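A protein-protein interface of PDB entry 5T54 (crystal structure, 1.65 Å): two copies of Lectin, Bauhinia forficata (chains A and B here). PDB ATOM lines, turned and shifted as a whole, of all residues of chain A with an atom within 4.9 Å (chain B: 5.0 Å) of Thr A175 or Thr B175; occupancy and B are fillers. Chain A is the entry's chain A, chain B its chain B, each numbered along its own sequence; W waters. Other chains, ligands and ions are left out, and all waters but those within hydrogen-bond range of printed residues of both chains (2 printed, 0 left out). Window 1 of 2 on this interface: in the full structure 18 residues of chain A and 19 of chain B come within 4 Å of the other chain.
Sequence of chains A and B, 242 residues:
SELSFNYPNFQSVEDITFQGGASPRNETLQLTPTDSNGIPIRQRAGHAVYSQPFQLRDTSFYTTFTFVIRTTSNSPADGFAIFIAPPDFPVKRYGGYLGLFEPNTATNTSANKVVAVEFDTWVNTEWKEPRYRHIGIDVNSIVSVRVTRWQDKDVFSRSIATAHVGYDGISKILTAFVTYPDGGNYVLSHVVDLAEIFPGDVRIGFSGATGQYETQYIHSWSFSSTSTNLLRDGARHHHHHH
The side-chain hydroxyl (OG1) of Thr A175 sits at hydrogen-bond distance from the side-chain hydroxyl (OG1) of Thr B175 (3.1 Å).
The backbone carbonyl oxygen of Gly B166 sits at hydrogen-bond distance from the backbone NH of Thr B175 (2.8 Å).
The side-chain hydroxyl (OG1) of Thr A175 lies within hydrogen-bond range of the side-chain hydroxyl (OG) of Ser A189, at 2.7 Å.
The backbone NH of His A164 lies within hydrogen-bond range of the backbone carbonyl oxygen of Phe A177 (2.8 Å).
The backbone carbonyl oxygen (O) of Thr A175 lies within hydrogen-bond range of the backbone NH (N) of Gly A166.
The side-chain hydroxyl (OG1) of Thr B175 sits at hydrogen-bond distance from the side-chain hydroxyl (OG) of Ser B189.
O of Phe B177 lies within hydrogen-bond range of N of His B164, at 2.8 Å.
His A164 touches His B164 (CE1 to CE1, 3.5 Å).
CB of His A164 touches CE2 of Phe B177, 3.6 Å away.
Ile A173 touches Ile B173 (CG2 to CG2, 3.9 Å).
Phe B177 touches Thr A175.
Phe A177 touches His B164.
Phe A177 touches Gly B166 (CZ to N, 3.5 Å).
Thr B175 touches Phe A177.
Phe A177 touches Phe B177 (CD2 to CE2, 3.5 Å).
CG2 of Ile B173 touches CB of Ser A189 (3.7 Å).
Thr B175 touches Ser A189.
Thr A175 touches just these residues of chain B: Thr B175, Phe B177 and Ser B189.
Thr B175 touches just these residues of chain A: Thr A175 (3.1 Å), Phe A177 (3.7 Å) and Ser A189 (3.8 Å).
Of the printed residues of chain A, Ser B189 touches Ile A173 and Thr A175.
Of the printed residues of chain A, Phe B177 touches His A164, Gly A166, Thr A175 and Phe A177.
Of the printed residues of chain B, Gly A166 touches Phe B177.
Of the printed residues of chain B, Phe A177 touches His B164 (3.7 Å), Gly B166 (3.5 Å), Thr B175 (3.7 Å) and Phe B177 (3.5 Å).
Leu A174 touches none of the printed residues of chain B.
Leu B188 touches none of the printed residues of chain A.
Hydrophobic or aromatic side chains of chain A that line the printed part of chain B: His A164, Ile A173 and Phe A177.
Of the 10 printed residues of chain B, 6 touch a printed residue of chain A.
Printed residues of chain B that touch a printed residue of chain A: His B164, Gly B166, Ile B173, Thr B175, Phe B177 and Ser B189.
Along chain B the printed residues that touch a printed residue of chain A span positions 164 to 189.
Among the printed residues, 14 pairs touch across the chains.
Among the printed residues, no Asp or Glu carboxylate lies within 4 Å of a Lys or Arg side-chain nitrogen of the other chain.
Gly A166 touches Phe B177, and with the chains exchanged Phe A177 touches Gly B166.
Thr A175 touches Phe B177, and with the chains exchanged Phe A177 touches Thr B175.
Thr A175 touches Ser B189, and with the chains exchanged Ser A189 touches Thr B175.
Phe A177 touches its own counterpart, Phe B177.
Positions printed for both chains: 164, 165, 166, 173, 174, 175, 176, 177, 188 and 189.
Of the 14 pairs that touch across the chains among the printed residues, 14 have their exchanged pair printed and touching as well.
Water W1 lies within hydrogen-bond range of the side-chain hydroxyl of Ser A189, the side-chain hydroxyl of Thr B175, the backbone carbonyl oxygen of Ile B173 and the backbone carbonyl oxygen of Gly B166.
Water W2 lies within hydrogen-bond range of the side-chain hydroxyl of Ser B189, the side-chain hydroxyl of Thr A175, the backbone carbonyl oxygen of Ile A173 and the backbone carbonyl oxygen of Gly A166.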
ATOM      1  N   HIS A 164       8.775 -20.605  -3.233  1.00  0.00           N
ATOM      2  CA  HIS A 164       8.374 -19.245  -3.564  1.00  0.00           C
ATOM      3  C   HIS A 164       9.291 -18.763  -4.638  1.00  0.00           C
ATOM      4  O   HIS A 164      10.533 -18.715  -4.447  1.00  0.00           O
ATOM      5  CB  HIS A 164       8.559 -18.279  -2.333  1.00  0.00           C
ATOM      6  CG  HIS A 164       7.871 -18.760  -1.124  1.00  0.00           C
ATOM      7  ND1 HIS A 164       6.587 -18.371  -0.765  1.00  0.00           N
ATOM      8  CD2 HIS A 164       8.299 -19.599  -0.178  1.00  0.00           C
ATOM      9  CE1 HIS A 164       6.263 -18.969   0.361  1.00  0.00           C
ATOM     10  NE2 HIS A 164       7.301 -19.708   0.740  1.00  0.00           N
ATOM     11  N   VAL A 165       8.742 -18.308  -5.738  1.00  0.00           N
ATOM     12  CA  VAL A 165       9.557 -17.798  -6.857  1.00  0.00           C
ATOM     13  C   VAL A 165       9.061 -16.435  -7.226  1.00  0.00           C
ATOM     14  O   VAL A 165       7.889 -16.230  -7.480  1.00  0.00           O
ATOM     15  CB  VAL A 165       9.580 -18.755  -8.079  1.00  0.00           C
ATOM     16  CG1 VAL A 165      10.410 -18.188  -9.204  1.00  0.00           C
ATOM     17  CG2 VAL A 165      10.158 -20.096  -7.670  1.00  0.00           C
ATOM     18  N   GLY A 166       9.958 -15.447  -7.232  1.00  0.00           N
ATOM     19  CA  GLY A 166       9.554 -14.084  -7.519  1.00  0.00           C
ATOM     20  C   GLY A 166      10.448 -13.477  -8.551  1.00  0.00           C
ATOM     21  O   GLY A 166      11.637 -13.825  -8.651  1.00  0.00           O
ATOM     22  N   ILE A 173      15.656  -9.275 -11.300  1.00  0.00           N
ATOM     23  CA  ILE A 173      16.190 -10.313 -10.406  1.00  0.00           C
ATOM     24  C   ILE A 173      15.135 -11.372 -10.180  1.00  0.00           C
ATOM     25  O   ILE A 173      13.968 -11.071  -9.831  1.00  0.00           O
ATOM     26  CB  ILE A 173      16.657  -9.679  -9.052  1.00  0.00           C
ATOM     27  CG1 ILE A 173      17.879  -8.834  -9.278  1.00  0.00           C
ATOM     28  CG2 ILE A 173      16.971 -10.818  -8.075  1.00  0.00           C
ATOM     29  CD1 ILE A 173      18.365  -8.029  -8.077  1.00  0.00           C
ATOM     30  N   LEU A 174      15.550 -12.639 -10.454  1.00  0.00           N
ATOM     31  CA  LEU A 174      14.729 -13.844 -10.203  1.00  0.00           C
ATOM     32  C   LEU A 174      15.219 -14.467  -8.917  1.00  0.00           C
ATOM     33  O   LEU A 174      16.443 -14.705  -8.765  1.00  0.00           O
ATOM     34  CB  LEU A 174      14.898 -14.795 -11.403  1.00  0.00           C
ATOM     35  CG  LEU A 174      14.062 -16.107 -11.323  1.00  0.00           C
ATOM     36  CD1 LEU A 174      12.575 -15.848 -11.420  1.00  0.00           C
ATOM     37  CD2 LEU A 174      14.497 -16.996 -12.479  1.00  0.00           C
ATOM     38  N   THR A 175      14.300 -14.786  -8.006  1.00  0.00           N
ATOM     39  CA  THR A 175      14.667 -15.358  -6.731  1.00  0.00           C
ATOM     40  C   THR A 175      13.812 -16.535  -6.409  1.00  0.00           C
ATOM     41  O   THR A 175      12.611 -16.486  -6.678  1.00  0.00           O
ATOM     42  CB  THR A 175      14.491 -14.327  -5.594  1.00  0.00           C
ATOM     43  OG1 THR A 175      15.389 -13.230  -5.830  1.00  0.00           O
ATOM     44  CG2 THR A 175      14.662 -14.860  -4.235  1.00  0.00           C
ATOM     45  N   ALA A 176      14.405 -17.608  -5.873  1.00  0.00           N
ATOM     46  CA  ALA A 176      13.652 -18.678  -5.261  1.00  0.00           C
ATOM     47  C   ALA A 176      13.999 -18.872  -3.775  1.00  0.00           C
ATOM     48  O   ALA A 176      15.188 -18.781  -3.407  1.00  0.00           O
ATOM     49  CB  ALA A 176      13.950 -19.998  -5.995  1.00  0.00           C
ATOM     50  N   PHE A 177      12.961 -19.047  -2.929  1.00  0.00           N
ATOM     51  CA  PHE A 177      13.070 -19.509  -1.573  1.00  0.00           C
ATOM     52  C   PHE A 177      12.335 -20.827  -1.487  1.00  0.00           C
ATOM     53  O   PHE A 177      11.171 -20.968  -1.898  1.00  0.00           O
ATOM     54  CB  PHE A 177      12.395 -18.569  -0.557  1.00  0.00           C
ATOM     55  CG  PHE A 177      12.846 -17.103  -0.568  1.00  0.00           C
ATOM     56  CD1 PHE A 177      14.123 -16.721  -0.854  1.00  0.00           C
ATOM     57  CD2 PHE A 177      11.919 -16.127  -0.182  1.00  0.00           C
ATOM     58  CE1 PHE A 177      14.482 -15.393  -0.795  1.00  0.00           C
ATOM     59  CE2 PHE A 177      12.284 -14.788  -0.101  1.00  0.00           C
ATOM     60  CZ  PHE A 177      13.592 -14.428  -0.401  1.00  0.00           C
ATOM     61  N   LEU A 188      18.160 -18.720  -3.556  1.00  0.00           N
ATOM     62  CA  LEU A 188      18.940 -18.471  -4.789  1.00  0.00           C
ATOM     63  C   LEU A 188      18.402 -17.276  -5.522  1.00  0.00           C
ATOM     64  O   LEU A 188      17.210 -17.241  -5.747  1.00  0.00           O
ATOM     65  CB  LEU A 188      18.751 -19.611  -5.832  1.00  0.00           C
ATOM     66  CG  LEU A 188      19.173 -20.977  -5.565  1.00  0.00           C
ATOM     67  CD1 LEU A 188      19.078 -21.858  -6.790  1.00  0.00           C
ATOM     68  CD2 LEU A 188      20.581 -20.889  -5.063  1.00  0.00           C
ATOM     69  N   SER A 189      19.274 -16.403  -6.036  1.00  0.00           N
ATOM     70  CA  SER A 189      18.866 -15.240  -6.813  1.00  0.00           C
ATOM     71  C   SER A 189      19.814 -15.041  -7.953  1.00  0.00           C
ATOM     72  O   SER A 189      20.998 -15.407  -7.828  1.00  0.00           O
ATOM     73  CB  SER A 189      18.844 -13.927  -5.933  1.00  0.00           C
ATOM     74  OG  SER A 189      17.852 -14.022  -4.923  1.00  0.00           O
ATOM     75  N   HIS B 164       8.686 -12.703   3.812  1.00  0.00           N
ATOM     76  CA  HIS B 164       9.854 -13.595   3.574  1.00  0.00           C
ATOM     77  C   HIS B 164      11.057 -12.725   3.146  1.00  0.00           C
ATOM     78  O   HIS B 164      10.968 -11.994   2.168  1.00  0.00           O
ATOM     79  CB  HIS B 164       9.539 -14.625   2.441  1.00  0.00           C
ATOM     80  CG  HIS B 164       8.291 -15.367   2.611  1.00  0.00           C
ATOM     81  ND1 HIS B 164       8.241 -16.609   3.201  1.00  0.00           N
ATOM     82  CD2 HIS B 164       7.047 -15.096   2.213  1.00  0.00           C
ATOM     83  CE1 HIS B 164       7.001 -17.043   3.208  1.00  0.00           C
ATOM     84  NE2 HIS B 164       6.245 -16.134   2.631  1.00  0.00           N
ATOM     85  N   VAL B 165      12.168 -12.761   3.875  1.00  0.00           N
ATOM     86  CA  VAL B 165      13.335 -11.979   3.469  1.00  0.00           C
ATOM     87  C   VAL B 165      14.491 -12.927   3.367  1.00  0.00           C
ATOM     88  O   VAL B 165      14.777 -13.715   4.265  1.00  0.00           O
ATOM     89  CB  VAL B 165      13.614 -10.873   4.498  1.00  0.00           C
ATOM     90  CG1 VAL B 165      14.938 -10.147   4.234  1.00  0.00           C
ATOM     91  CG2 VAL B 165      12.393  -9.930   4.576  1.00  0.00           C
ATOM     92  N   GLY B 166      15.184 -12.882   2.255  1.00  0.00           N
ATOM     93  CA  GLY B 166      16.281 -13.771   1.965  1.00  0.00           C
ATOM     94  C   GLY B 166      17.483 -13.030   1.477  1.00  0.00           C
ATOM     95  O   GLY B 166      17.389 -12.034   0.743  1.00  0.00           O
ATOM     96  N   ILE B 173      22.494 -10.689  -3.082  1.00  0.00           N
ATOM     97  CA  ILE B 173      21.150 -10.164  -3.401  1.00  0.00           C
ATOM     98  C   ILE B 173      20.266 -10.357  -2.190  1.00  0.00           C
ATOM     99  O   ILE B 173      20.155 -11.490  -1.660  1.00  0.00           O
ATOM    100  CB  ILE B 173      20.521 -10.873  -4.615  1.00  0.00           C
ATOM    101  CG1 ILE B 173      21.310 -10.451  -5.852  1.00  0.00           C
ATOM    102  CG2 ILE B 173      19.066 -10.449  -4.770  1.00  0.00           C
ATOM    103  CD1 ILE B 173      20.905 -11.089  -7.176  1.00  0.00           C
ATOM    104  N   LEU B 174      19.682  -9.271  -1.723  1.00  0.00           N
ATOM    105  CA  LEU B 174      18.676  -9.262  -0.706  1.00  0.00           C
ATOM    106  C   LEU B 174      17.269  -9.116  -1.380  1.00  0.00           C
ATOM    107  O   LEU B 174      17.032  -8.251  -2.254  1.00  0.00           O
ATOM    108  CB  LEU B 174      18.910  -8.010   0.129  1.00  0.00           C
ATOM    109  CG  LEU B 174      18.016  -7.890   1.379  1.00  0.00           C
ATOM    110  CD1 LEU B 174      18.274  -9.030   2.364  1.00  0.00           C
ATOM    111  CD2 LEU B 174      18.235  -6.556   2.069  1.00  0.00           C
ATOM    112  N   THR B 175      16.396 -10.013  -0.974  1.00  0.00           N
ATOM    113  CA  THR B 175      15.002 -10.069  -1.536  1.00  0.00           C
ATOM    114  C   THR B 175      13.933 -10.134  -0.449  1.00  0.00           C
ATOM    115  O   THR B 175      14.106 -10.881   0.544  1.00  0.00           O
ATOM    116  CB  THR B 175      14.883 -11.343  -2.403  1.00  0.00           C
ATOM    117  OG1 THR B 175      15.756 -11.179  -3.518  1.00  0.00           O
ATOM    118  CG2 THR B 175      13.359 -11.502  -2.919  1.00  0.00           C
ATOM    119  N   ALA B 176      12.812  -9.395  -0.613  1.00  0.00           N
ATOM    120  CA  ALA B 176      11.629  -9.500   0.185  1.00  0.00           C
ATOM    121  C   ALA B 176      10.433  -9.913  -0.718  1.00  0.00           C
ATOM    122  O   ALA B 176      10.215  -9.356  -1.786  1.00  0.00           O
ATOM    123  CB  ALA B 176      11.257  -8.230   0.913  1.00  0.00           C
ATOM    124  N   PHE B 177       9.713 -10.892  -0.220  1.00  0.00           N
ATOM    125  CA  PHE B 177       8.365 -11.238  -0.678  1.00  0.00           C
ATOM    126  C   PHE B 177       7.379 -10.972   0.443  1.00  0.00           C
ATOM    127  O   PHE B 177       7.543 -11.463   1.543  1.00  0.00           O
ATOM    128  CB  PHE B 177       8.207 -12.748  -1.092  1.00  0.00           C
ATOM    129  CG  PHE B 177       9.178 -13.238  -2.115  1.00  0.00           C
ATOM    130  CD1 PHE B 177       9.690 -12.462  -3.154  1.00  0.00           C
ATOM    131  CD2 PHE B 177       9.444 -14.618  -2.138  1.00  0.00           C
ATOM    132  CE1 PHE B 177      10.575 -13.008  -4.104  1.00  0.00           C
ATOM    133  CE2 PHE B 177      10.263 -15.176  -3.075  1.00  0.00           C
ATOM    134  CZ  PHE B 177      10.855 -14.366  -4.091  1.00  0.00           C
ATOM    135  N   LEU B 188      10.422  -7.387  -3.926  1.00  0.00           N
ATOM    136  CA  LEU B 188      11.546  -6.472  -4.071  1.00  0.00           C
ATOM    137  C   LEU B 188      12.861  -7.106  -3.877  1.00  0.00           C
ATOM    138  O   LEU B 188      13.073  -7.824  -2.900  1.00  0.00           O
ATOM    139  CB  LEU B 188      11.539  -5.317  -3.033  1.00  0.00           C
ATOM    140  CG  LEU B 188      10.407  -4.455  -2.618  1.00  0.00           C
ATOM    141  CD1 LEU B 188      11.061  -3.390  -1.749  1.00  0.00           C
ATOM    142  CD2 LEU B 188       9.768  -3.776  -3.796  1.00  0.00           C
ATOM    143  N   SER B 189      13.783  -6.726  -4.740  1.00  0.00           N
ATOM    144  CA  SER B 189      15.173  -7.262  -4.717  1.00  0.00           C
ATOM    145  C   SER B 189      16.191  -6.199  -5.001  1.00  0.00           C
ATOM    146  O   SER B 189      15.930  -5.262  -5.760  1.00  0.00           O
ATOM    147  CB  SER B 189      15.373  -8.427  -5.756  1.00  0.00           C
ATOM    148  OG  SER B 189      14.616  -9.567  -5.376  1.00  0.00           O
HETATM  149  O   HOH W   1      17.726 -12.909  -2.459  1.00  0.00           O
HETATM  150  O   HOH W   2      13.461 -11.462  -6.948  1.00  0.00           O
